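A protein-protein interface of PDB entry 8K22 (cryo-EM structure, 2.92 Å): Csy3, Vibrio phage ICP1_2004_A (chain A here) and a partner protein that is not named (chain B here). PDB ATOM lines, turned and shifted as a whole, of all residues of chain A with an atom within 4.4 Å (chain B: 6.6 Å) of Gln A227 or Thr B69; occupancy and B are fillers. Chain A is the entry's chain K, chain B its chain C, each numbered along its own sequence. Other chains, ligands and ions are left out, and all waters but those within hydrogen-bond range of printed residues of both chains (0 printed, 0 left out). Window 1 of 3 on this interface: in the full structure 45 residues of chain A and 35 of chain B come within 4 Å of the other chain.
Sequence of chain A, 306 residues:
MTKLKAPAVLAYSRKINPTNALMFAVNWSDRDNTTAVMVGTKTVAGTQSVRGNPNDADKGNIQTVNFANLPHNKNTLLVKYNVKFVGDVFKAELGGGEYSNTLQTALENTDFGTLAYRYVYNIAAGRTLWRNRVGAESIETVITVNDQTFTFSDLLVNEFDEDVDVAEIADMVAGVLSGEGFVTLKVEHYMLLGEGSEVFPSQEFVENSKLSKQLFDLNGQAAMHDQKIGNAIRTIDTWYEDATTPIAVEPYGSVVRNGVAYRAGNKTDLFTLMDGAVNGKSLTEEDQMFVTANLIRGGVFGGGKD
OD2 of Asp A226 sits close to N of Gly B14 (3.4 Å).
The guanidinium group (NH2) of Arg B60 lies within salt-bridge range of the side-chain carboxylate (OD1) of Asp A226 (3.2 Å).
NH2 of Arg B60 is in hydrogen-bond range of OE1 of Gln A227, 2.6 Å away.
The backbone NH of Arg B60 lies within hydrogen-bond range of the backbone carbonyl oxygen of Leu B93 (2.9 Å).
The side-chain carboxylate (OD1) of Asp A226 sits close to the side-chain amide oxygen (OE1) of Gln A227 (2.9 Å).
The side-chain hydroxyl (OG1) of Thr B69 is in hydrogen-bond range of the backbone carbonyl oxygen (O) of Lys B91, at 3.2 Å.
O of Arg B60 lies within hydrogen-bond range of N of Ser B67 (2.5 Å).
His A225 touches Arg B60.
Thr B69 touches Gln A227 (CG2 to NE2, 3.4 Å).
Gln A227 touches Leu B93 (NE2 to CD1, 3.6 Å).
Of chain A, only Gln A227 (3.4 Å) comes within 4 Å of Thr B69.
Of the printed residues of chain A, Arg B60 touches His A225, Asp A226 and Gln A227.
Of the printed residues of chain A, Leu B93 touches Gln A227 (3.6 Å).
Printed residues of chain B within 4 Å of Asp A226: Gly B14 (3.3 Å) and Arg B60 (3.2 Å).
Of the printed residues of chain B, His A225 touches Arg B60 (3.2 Å).
Ser B86 touches none of the printed residues of chain A.
Pro B92 touches none of the printed residues of chain A.
The nearest residue of chain B that does not touch Gln A227 is Lys B70 (5.3 Å).
The nearest printed residue of chain A that does not touch Thr B69 is His A225 (7.7 Å).
Hydrophobic or aromatic side chains of chain B that line the printed part of chain A: Leu B93.
Of the 7 printed residues of chain A, 3 touch a printed residue of chain B.
Hydrophobic or aromatic side chains of chain A within 4 Å of the printed part of chain B: His A225.
Among the printed residues, 6 pairs touch across the chains.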
ATOM      1  N   HIS A 225      -0.664   9.545 -19.433  1.00  0.00           N
ATOM      2  CA  HIS A 225      -0.909  10.701 -18.585  1.00  0.00           C
ATOM      3  C   HIS A 225      -2.264  11.313 -18.905  1.00  0.00           C
ATOM      4  O   HIS A 225      -2.708  11.300 -20.054  1.00  0.00           O
ATOM      5  CB  HIS A 225       0.190  11.741 -18.780  1.00  0.00           C
ATOM      6  CG  HIS A 225       1.518  11.332 -18.225  1.00  0.00           C
ATOM      7  ND1 HIS A 225       2.711  11.772 -18.753  1.00  0.00           N
ATOM      8  CD2 HIS A 225       1.841  10.525 -17.189  1.00  0.00           C
ATOM      9  CE1 HIS A 225       3.713  11.255 -18.066  1.00  0.00           C
ATOM     10  NE2 HIS A 225       3.212  10.493 -17.111  1.00  0.00           N
ATOM     11  N   ASP A 226      -2.938  11.822 -17.871  1.00  0.00           N
ATOM     12  CA  ASP A 226      -4.255  12.415 -18.079  1.00  0.00           C
ATOM     13  C   ASP A 226      -4.160  13.724 -18.850  1.00  0.00           C
ATOM     14  O   ASP A 226      -5.010  14.010 -19.699  1.00  0.00           O
ATOM     15  CB  ASP A 226      -4.964  12.621 -16.742  1.00  0.00           C
ATOM     16  CG  ASP A 226      -4.078  13.262 -15.699  1.00  0.00           C
ATOM     17  OD1 ASP A 226      -2.875  13.448 -15.966  1.00  0.00           O
ATOM     18  OD2 ASP A 226      -4.585  13.567 -14.601  1.00  0.00           O
ATOM     19  N   GLN A 227      -3.122  14.523 -18.593  1.00  0.00           N
ATOM     20  CA  GLN A 227      -2.965  15.765 -19.340  1.00  0.00           C
ATOM     21  C   GLN A 227      -2.560  15.514 -20.786  1.00  0.00           C
ATOM     22  O   GLN A 227      -2.800  16.373 -21.639  1.00  0.00           O
ATOM     23  CB  GLN A 227      -1.953  16.682 -18.651  1.00  0.00           C
ATOM     24  CG  GLN A 227      -0.512  16.275 -18.815  1.00  0.00           C
ATOM     25  CD  GLN A 227       0.039  15.557 -17.608  1.00  0.00           C
ATOM     26  OE1 GLN A 227      -0.512  14.555 -17.166  1.00  0.00           O
ATOM     27  NE2 GLN A 227       1.139  16.062 -17.070  1.00  0.00           N
ATOM     28  N   LYS A 228      -2.000  14.340 -21.084  1.00  0.00           N
ATOM     29  CA  LYS A 228      -1.758  13.941 -22.466  1.00  0.00           C
ATOM     30  C   LYS A 228      -3.069  13.775 -23.231  1.00  0.00           C
ATOM     31  O   LYS A 228      -3.237  14.317 -24.333  1.00  0.00           O
ATOM     32  CB  LYS A 228      -0.951  12.646 -22.482  1.00  0.00           C
ATOM     33  CG  LYS A 228      -0.390  12.308 -23.818  1.00  0.00           C
ATOM     34  CD  LYS A 228       1.050  11.905 -23.803  1.00  0.00           C
ATOM     35  CE  LYS A 228       1.476  11.593 -25.222  1.00  0.00           C
ATOM     36  NZ  LYS A 228       1.382  12.791 -26.096  1.00  0.00           N
ATOM     37  N   ILE A 229      -4.025  13.056 -22.640  1.00  0.00           N
ATOM     38  CA  ILE A 229      -5.340  12.893 -23.254  1.00  0.00           C
ATOM     39  C   ILE A 229      -6.083  14.223 -23.291  1.00  0.00           C
ATOM     40  O   ILE A 229      -6.836  14.501 -24.232  1.00  0.00           O
ATOM     41  CB  ILE A 229      -6.127  11.810 -22.499  1.00  0.00           C
ATOM     42  CG1 ILE A 229      -5.304  10.534 -22.449  1.00  0.00           C
ATOM     43  CG2 ILE A 229      -7.451  11.506 -23.169  1.00  0.00           C
ATOM     44  CD1 ILE A 229      -5.427   9.835 -21.167  1.00  0.00           C
ATOM     45  N   GLY A 230      -5.874  15.071 -22.281  1.00  0.00           N
ATOM     46  CA  GLY A 230      -6.448  16.408 -22.312  1.00  0.00           C
ATOM     47  C   GLY A 230      -5.904  17.257 -23.445  1.00  0.00           C
ATOM     48  O   GLY A 230      -6.632  18.055 -24.039  1.00  0.00           O
ATOM     49  N   ASN A 231      -4.617  17.094 -23.757  1.00  0.00           N
ATOM     50  CA  ASN A 231      -4.050  17.723 -24.944  1.00  0.00           C
ATOM     51  C   ASN A 231      -4.633  17.134 -26.219  1.00  0.00           C
ATOM     52  O   ASN A 231      -4.776  17.844 -27.219  1.00  0.00           O
ATOM     53  CB  ASN A 231      -2.531  17.569 -24.941  1.00  0.00           C
ATOM     54  CG  ASN A 231      -1.863  18.368 -26.036  1.00  0.00           C
ATOM     55  OD1 ASN A 231      -1.586  19.554 -25.873  1.00  0.00           O
ATOM     56  ND2 ASN A 231      -1.593  17.718 -27.161  1.00  0.00           N
ATOM     57  N   GLY B  14      -3.638  12.877 -11.432  1.00  0.00           N
ATOM     58  CA  GLY B  14      -3.299  14.269 -11.623  1.00  0.00           C
ATOM     59  C   GLY B  14      -3.211  15.057 -10.340  1.00  0.00           C
ATOM     60  O   GLY B  14      -3.336  16.287 -10.372  1.00  0.00           O
ATOM     61  N   ARG B  60       4.406  10.342  -9.692  1.00  0.00           N
ATOM     62  CA  ARG B  60       4.928  10.170 -11.040  1.00  0.00           C
ATOM     63  C   ARG B  60       6.392  10.583 -11.088  1.00  0.00           C
ATOM     64  O   ARG B  60       6.731  11.732 -10.787  1.00  0.00           O
ATOM     65  CB  ARG B  60       4.103  10.985 -12.028  1.00  0.00           C
ATOM     66  CG  ARG B  60       2.730  10.407 -12.255  1.00  0.00           C
ATOM     67  CD  ARG B  60       1.662  11.465 -12.394  1.00  0.00           C
ATOM     68  NE  ARG B  60       1.459  11.886 -13.773  1.00  0.00           N
ATOM     69  CZ  ARG B  60       0.311  12.353 -14.242  1.00  0.00           C
ATOM     70  NH1 ARG B  60      -0.763  12.443 -13.476  1.00  0.00           N
ATOM     71  NH2 ARG B  60       0.238  12.741 -15.511  1.00  0.00           N
ATOM     72  N   SER B  67       8.430  13.258 -11.852  1.00  0.00           N
ATOM     73  CA  SER B  67       8.252  13.612 -13.254  1.00  0.00           C
ATOM     74  C   SER B  67       7.667  15.011 -13.320  1.00  0.00           C
ATOM     75  O   SER B  67       6.545  15.243 -12.863  1.00  0.00           O
ATOM     76  CB  SER B  67       7.342  12.614 -13.959  1.00  0.00           C
ATOM     77  OG  SER B  67       5.988  13.019 -13.870  1.00  0.00           O
ATOM     78  N   VAL B  68       8.425  15.947 -13.879  1.00  0.00           N
ATOM     79  CA  VAL B  68       7.937  17.312 -13.978  1.00  0.00           C
ATOM     80  C   VAL B  68       6.906  17.406 -15.098  1.00  0.00           C
ATOM     81  O   VAL B  68       6.818  16.551 -15.982  1.00  0.00           O
ATOM     82  CB  VAL B  68       9.092  18.310 -14.180  1.00  0.00           C
ATOM     83  CG1 VAL B  68      10.253  17.966 -13.261  1.00  0.00           C
ATOM     84  CG2 VAL B  68       9.544  18.336 -15.618  1.00  0.00           C
ATOM     85  N   THR B  69       6.092  18.451 -15.032  1.00  0.00           N
ATOM     86  CA  THR B  69       5.005  18.644 -15.975  1.00  0.00           C
ATOM     87  C   THR B  69       5.468  19.566 -17.093  1.00  0.00           C
ATOM     88  O   THR B  69       6.067  20.612 -16.827  1.00  0.00           O
ATOM     89  CB  THR B  69       3.788  19.234 -15.264  1.00  0.00           C
ATOM     90  OG1 THR B  69       3.609  18.575 -14.006  1.00  0.00           O
ATOM     91  CG2 THR B  69       2.545  19.034 -16.091  1.00  0.00           C
ATOM     92  N   LYS B  70       5.217  19.165 -18.337  1.00  0.00           N
ATOM     93  CA  LYS B  70       5.549  20.007 -19.482  1.00  0.00           C
ATOM     94  C   LYS B  70       4.630  21.217 -19.487  1.00  0.00           C
ATOM     95  O   LYS B  70       3.447  21.105 -19.814  1.00  0.00           O
ATOM     96  CB  LYS B  70       5.418  19.225 -20.784  1.00  0.00           C
ATOM     97  CG  LYS B  70       6.461  18.149 -20.965  1.00  0.00           C
ATOM     98  CD  LYS B  70       7.301  18.387 -22.207  1.00  0.00           C
ATOM     99  CE  LYS B  70       6.440  18.524 -23.450  1.00  0.00           C
ATOM    100  NZ  LYS B  70       7.251  18.862 -24.651  1.00  0.00           N
ATOM    101  N   PHE B  71       5.177  22.372 -19.122  1.00  0.00           N
ATOM    102  CA  PHE B  71       4.379  23.577 -18.975  1.00  0.00           C
ATOM    103  C   PHE B  71       3.913  24.086 -20.331  1.00  0.00           C
ATOM    104  O   PHE B  71       4.541  23.842 -21.364  1.00  0.00           O
ATOM    105  CB  PHE B  71       5.183  24.661 -18.260  1.00  0.00           C
ATOM    106  CG  PHE B  71       5.000  24.668 -16.771  1.00  0.00           C
ATOM    107  CD1 PHE B  71       4.850  23.484 -16.072  1.00  0.00           C
ATOM    108  CD2 PHE B  71       4.977  25.860 -16.070  1.00  0.00           C
ATOM    109  CE1 PHE B  71       4.685  23.486 -14.706  1.00  0.00           C
ATOM    110  CE2 PHE B  71       4.807  25.868 -14.704  1.00  0.00           C
ATOM    111  CZ  PHE B  71       4.662  24.680 -14.020  1.00  0.00           C
ATOM    112  N   ALA B  72       2.785  24.780 -20.321  1.00  0.00           N
ATOM    113  CA  ALA B  72       2.219  25.378 -21.515  1.00  0.00           C
ATOM    114  C   ALA B  72       2.360  26.890 -21.437  1.00  0.00           C
ATOM    115  O   ALA B  72       2.278  27.483 -20.358  1.00  0.00           O
ATOM    116  CB  ALA B  72       0.747  24.997 -21.682  1.00  0.00           C
ATOM    117  N   SER B  86       8.175  25.850 -22.885  1.00  0.00           N
ATOM    118  CA  SER B  86       7.868  26.682 -21.736  1.00  0.00           C
ATOM    119  C   SER B  86       8.734  26.272 -20.550  1.00  0.00           C
ATOM    120  O   SER B  86       9.022  25.084 -20.375  1.00  0.00           O
ATOM    121  CB  SER B  86       6.393  26.572 -21.369  1.00  0.00           C
ATOM    122  OG  SER B  86       6.099  27.333 -20.212  1.00  0.00           O
ATOM    123  N   PRO B  87       9.195  27.231 -19.750  1.00  0.00           N
ATOM    124  CA  PRO B  87       9.982  26.888 -18.563  1.00  0.00           C
ATOM    125  C   PRO B  87       9.138  26.173 -17.523  1.00  0.00           C
ATOM    126  O   PRO B  87       7.940  26.428 -17.385  1.00  0.00           O
ATOM    127  CB  PRO B  87      10.466  28.248 -18.056  1.00  0.00           C
ATOM    128  CG  PRO B  87      10.345  29.152 -19.229  1.00  0.00           C
ATOM    129  CD  PRO B  87       9.154  28.681 -19.975  1.00  0.00           C
ATOM    130  N   ILE B  88       9.777  25.271 -16.792  1.00  0.00           N
ATOM    131  CA  ILE B  88       9.072  24.365 -15.895  1.00  0.00           C
ATOM    132  C   ILE B  88       9.220  24.861 -14.467  1.00  0.00           C
ATOM    133  O   ILE B  88      10.329  24.899 -13.925  1.00  0.00           O
ATOM    134  CB  ILE B  88       9.600  22.930 -16.027  1.00  0.00           C
ATOM    135  CG1 ILE B  88       9.749  22.538 -17.497  1.00  0.00           C
ATOM    136  CG2 ILE B  88       8.689  21.970 -15.290  1.00  0.00           C
ATOM    137  CD1 ILE B  88       8.454  22.480 -18.253  1.00  0.00           C
ATOM    138  N   GLN B  89       8.132  25.232 -13.876  1.00  0.00           N
ATOM    139  CA  GLN B  89       8.170  25.400 -12.438  1.00  0.00           C
ATOM    140  C   GLN B  89       7.874  24.069 -11.763  1.00  0.00           C
ATOM    141  O   GLN B  89       7.126  23.251 -12.306  1.00  0.00           O
ATOM    142  CB  GLN B  89       7.152  26.456 -11.985  1.00  0.00           C
ATOM    143  CG  GLN B  89       7.166  27.751 -12.796  1.00  0.00           C
ATOM    144  CD  GLN B  89       8.515  28.444 -12.838  1.00  0.00           C
ATOM    145  OE1 GLN B  89       9.310  28.359 -11.902  1.00  0.00           O
ATOM    146  NE2 GLN B  89       8.786  29.128 -13.943  1.00  0.00           N
ATOM    147  N   LYS B  91       6.174  21.329 -10.085  1.00  0.00           N
ATOM    148  CA  LYS B  91       4.926  20.796  -9.543  1.00  0.00           C
ATOM    149  C   LYS B  91       4.871  19.306  -9.858  1.00  0.00           C
ATOM    150  O   LYS B  91       4.516  18.911 -10.980  1.00  0.00           O
ATOM    151  CB  LYS B  91       3.697  21.520 -10.086  1.00  0.00           C
ATOM    152  CG  LYS B  91       3.802  22.011 -11.510  1.00  0.00           C
ATOM    153  CD  LYS B  91       2.437  22.436 -12.006  1.00  0.00           C
ATOM    154  CE  LYS B  91       1.459  21.275 -12.022  1.00  0.00           C
ATOM    155  NZ  LYS B  91       0.135  21.691 -12.557  1.00  0.00           N
ATOM    156  N   PRO B  92       5.261  18.457  -8.913  1.00  0.00           N
ATOM    157  CA  PRO B  92       5.110  17.014  -9.110  1.00  0.00           C
ATOM    158  C   PRO B  92       3.650  16.602  -9.169  1.00  0.00           C
ATOM    159  O   PRO B  92       2.793  17.175  -8.496  1.00  0.00           O
ATOM    160  CB  PRO B  92       5.801  16.419  -7.882  1.00  0.00           C
ATOM    161  CG  PRO B  92       6.753  17.468  -7.453  1.00  0.00           C
ATOM    162  CD  PRO B  92       6.071  18.764  -7.724  1.00  0.00           C
ATOM    163  N   LEU B  93       3.380  15.595  -9.987  1.00  0.00           N
ATOM    164  CA  LEU B  93       2.052  15.025 -10.120  1.00  0.00           C
ATOM    165  C   LEU B  93       2.060  13.595  -9.599  1.00  0.00           C
ATOM    166  O   LEU B  93       3.103  12.941  -9.531  1.00  0.00           O
ATOM    167  CB  LEU B  93       1.581  15.060 -11.577  1.00  0.00           C
ATOM    168  CG  LEU B  93       1.051  16.394 -12.098  1.00  0.00           C
ATOM    169  CD1 LEU B  93       0.485  16.224 -13.493  1.00  0.00           C
ATOM    170  CD2 LEU B  93       0.005  16.967 -11.165  1.00  0.00           C
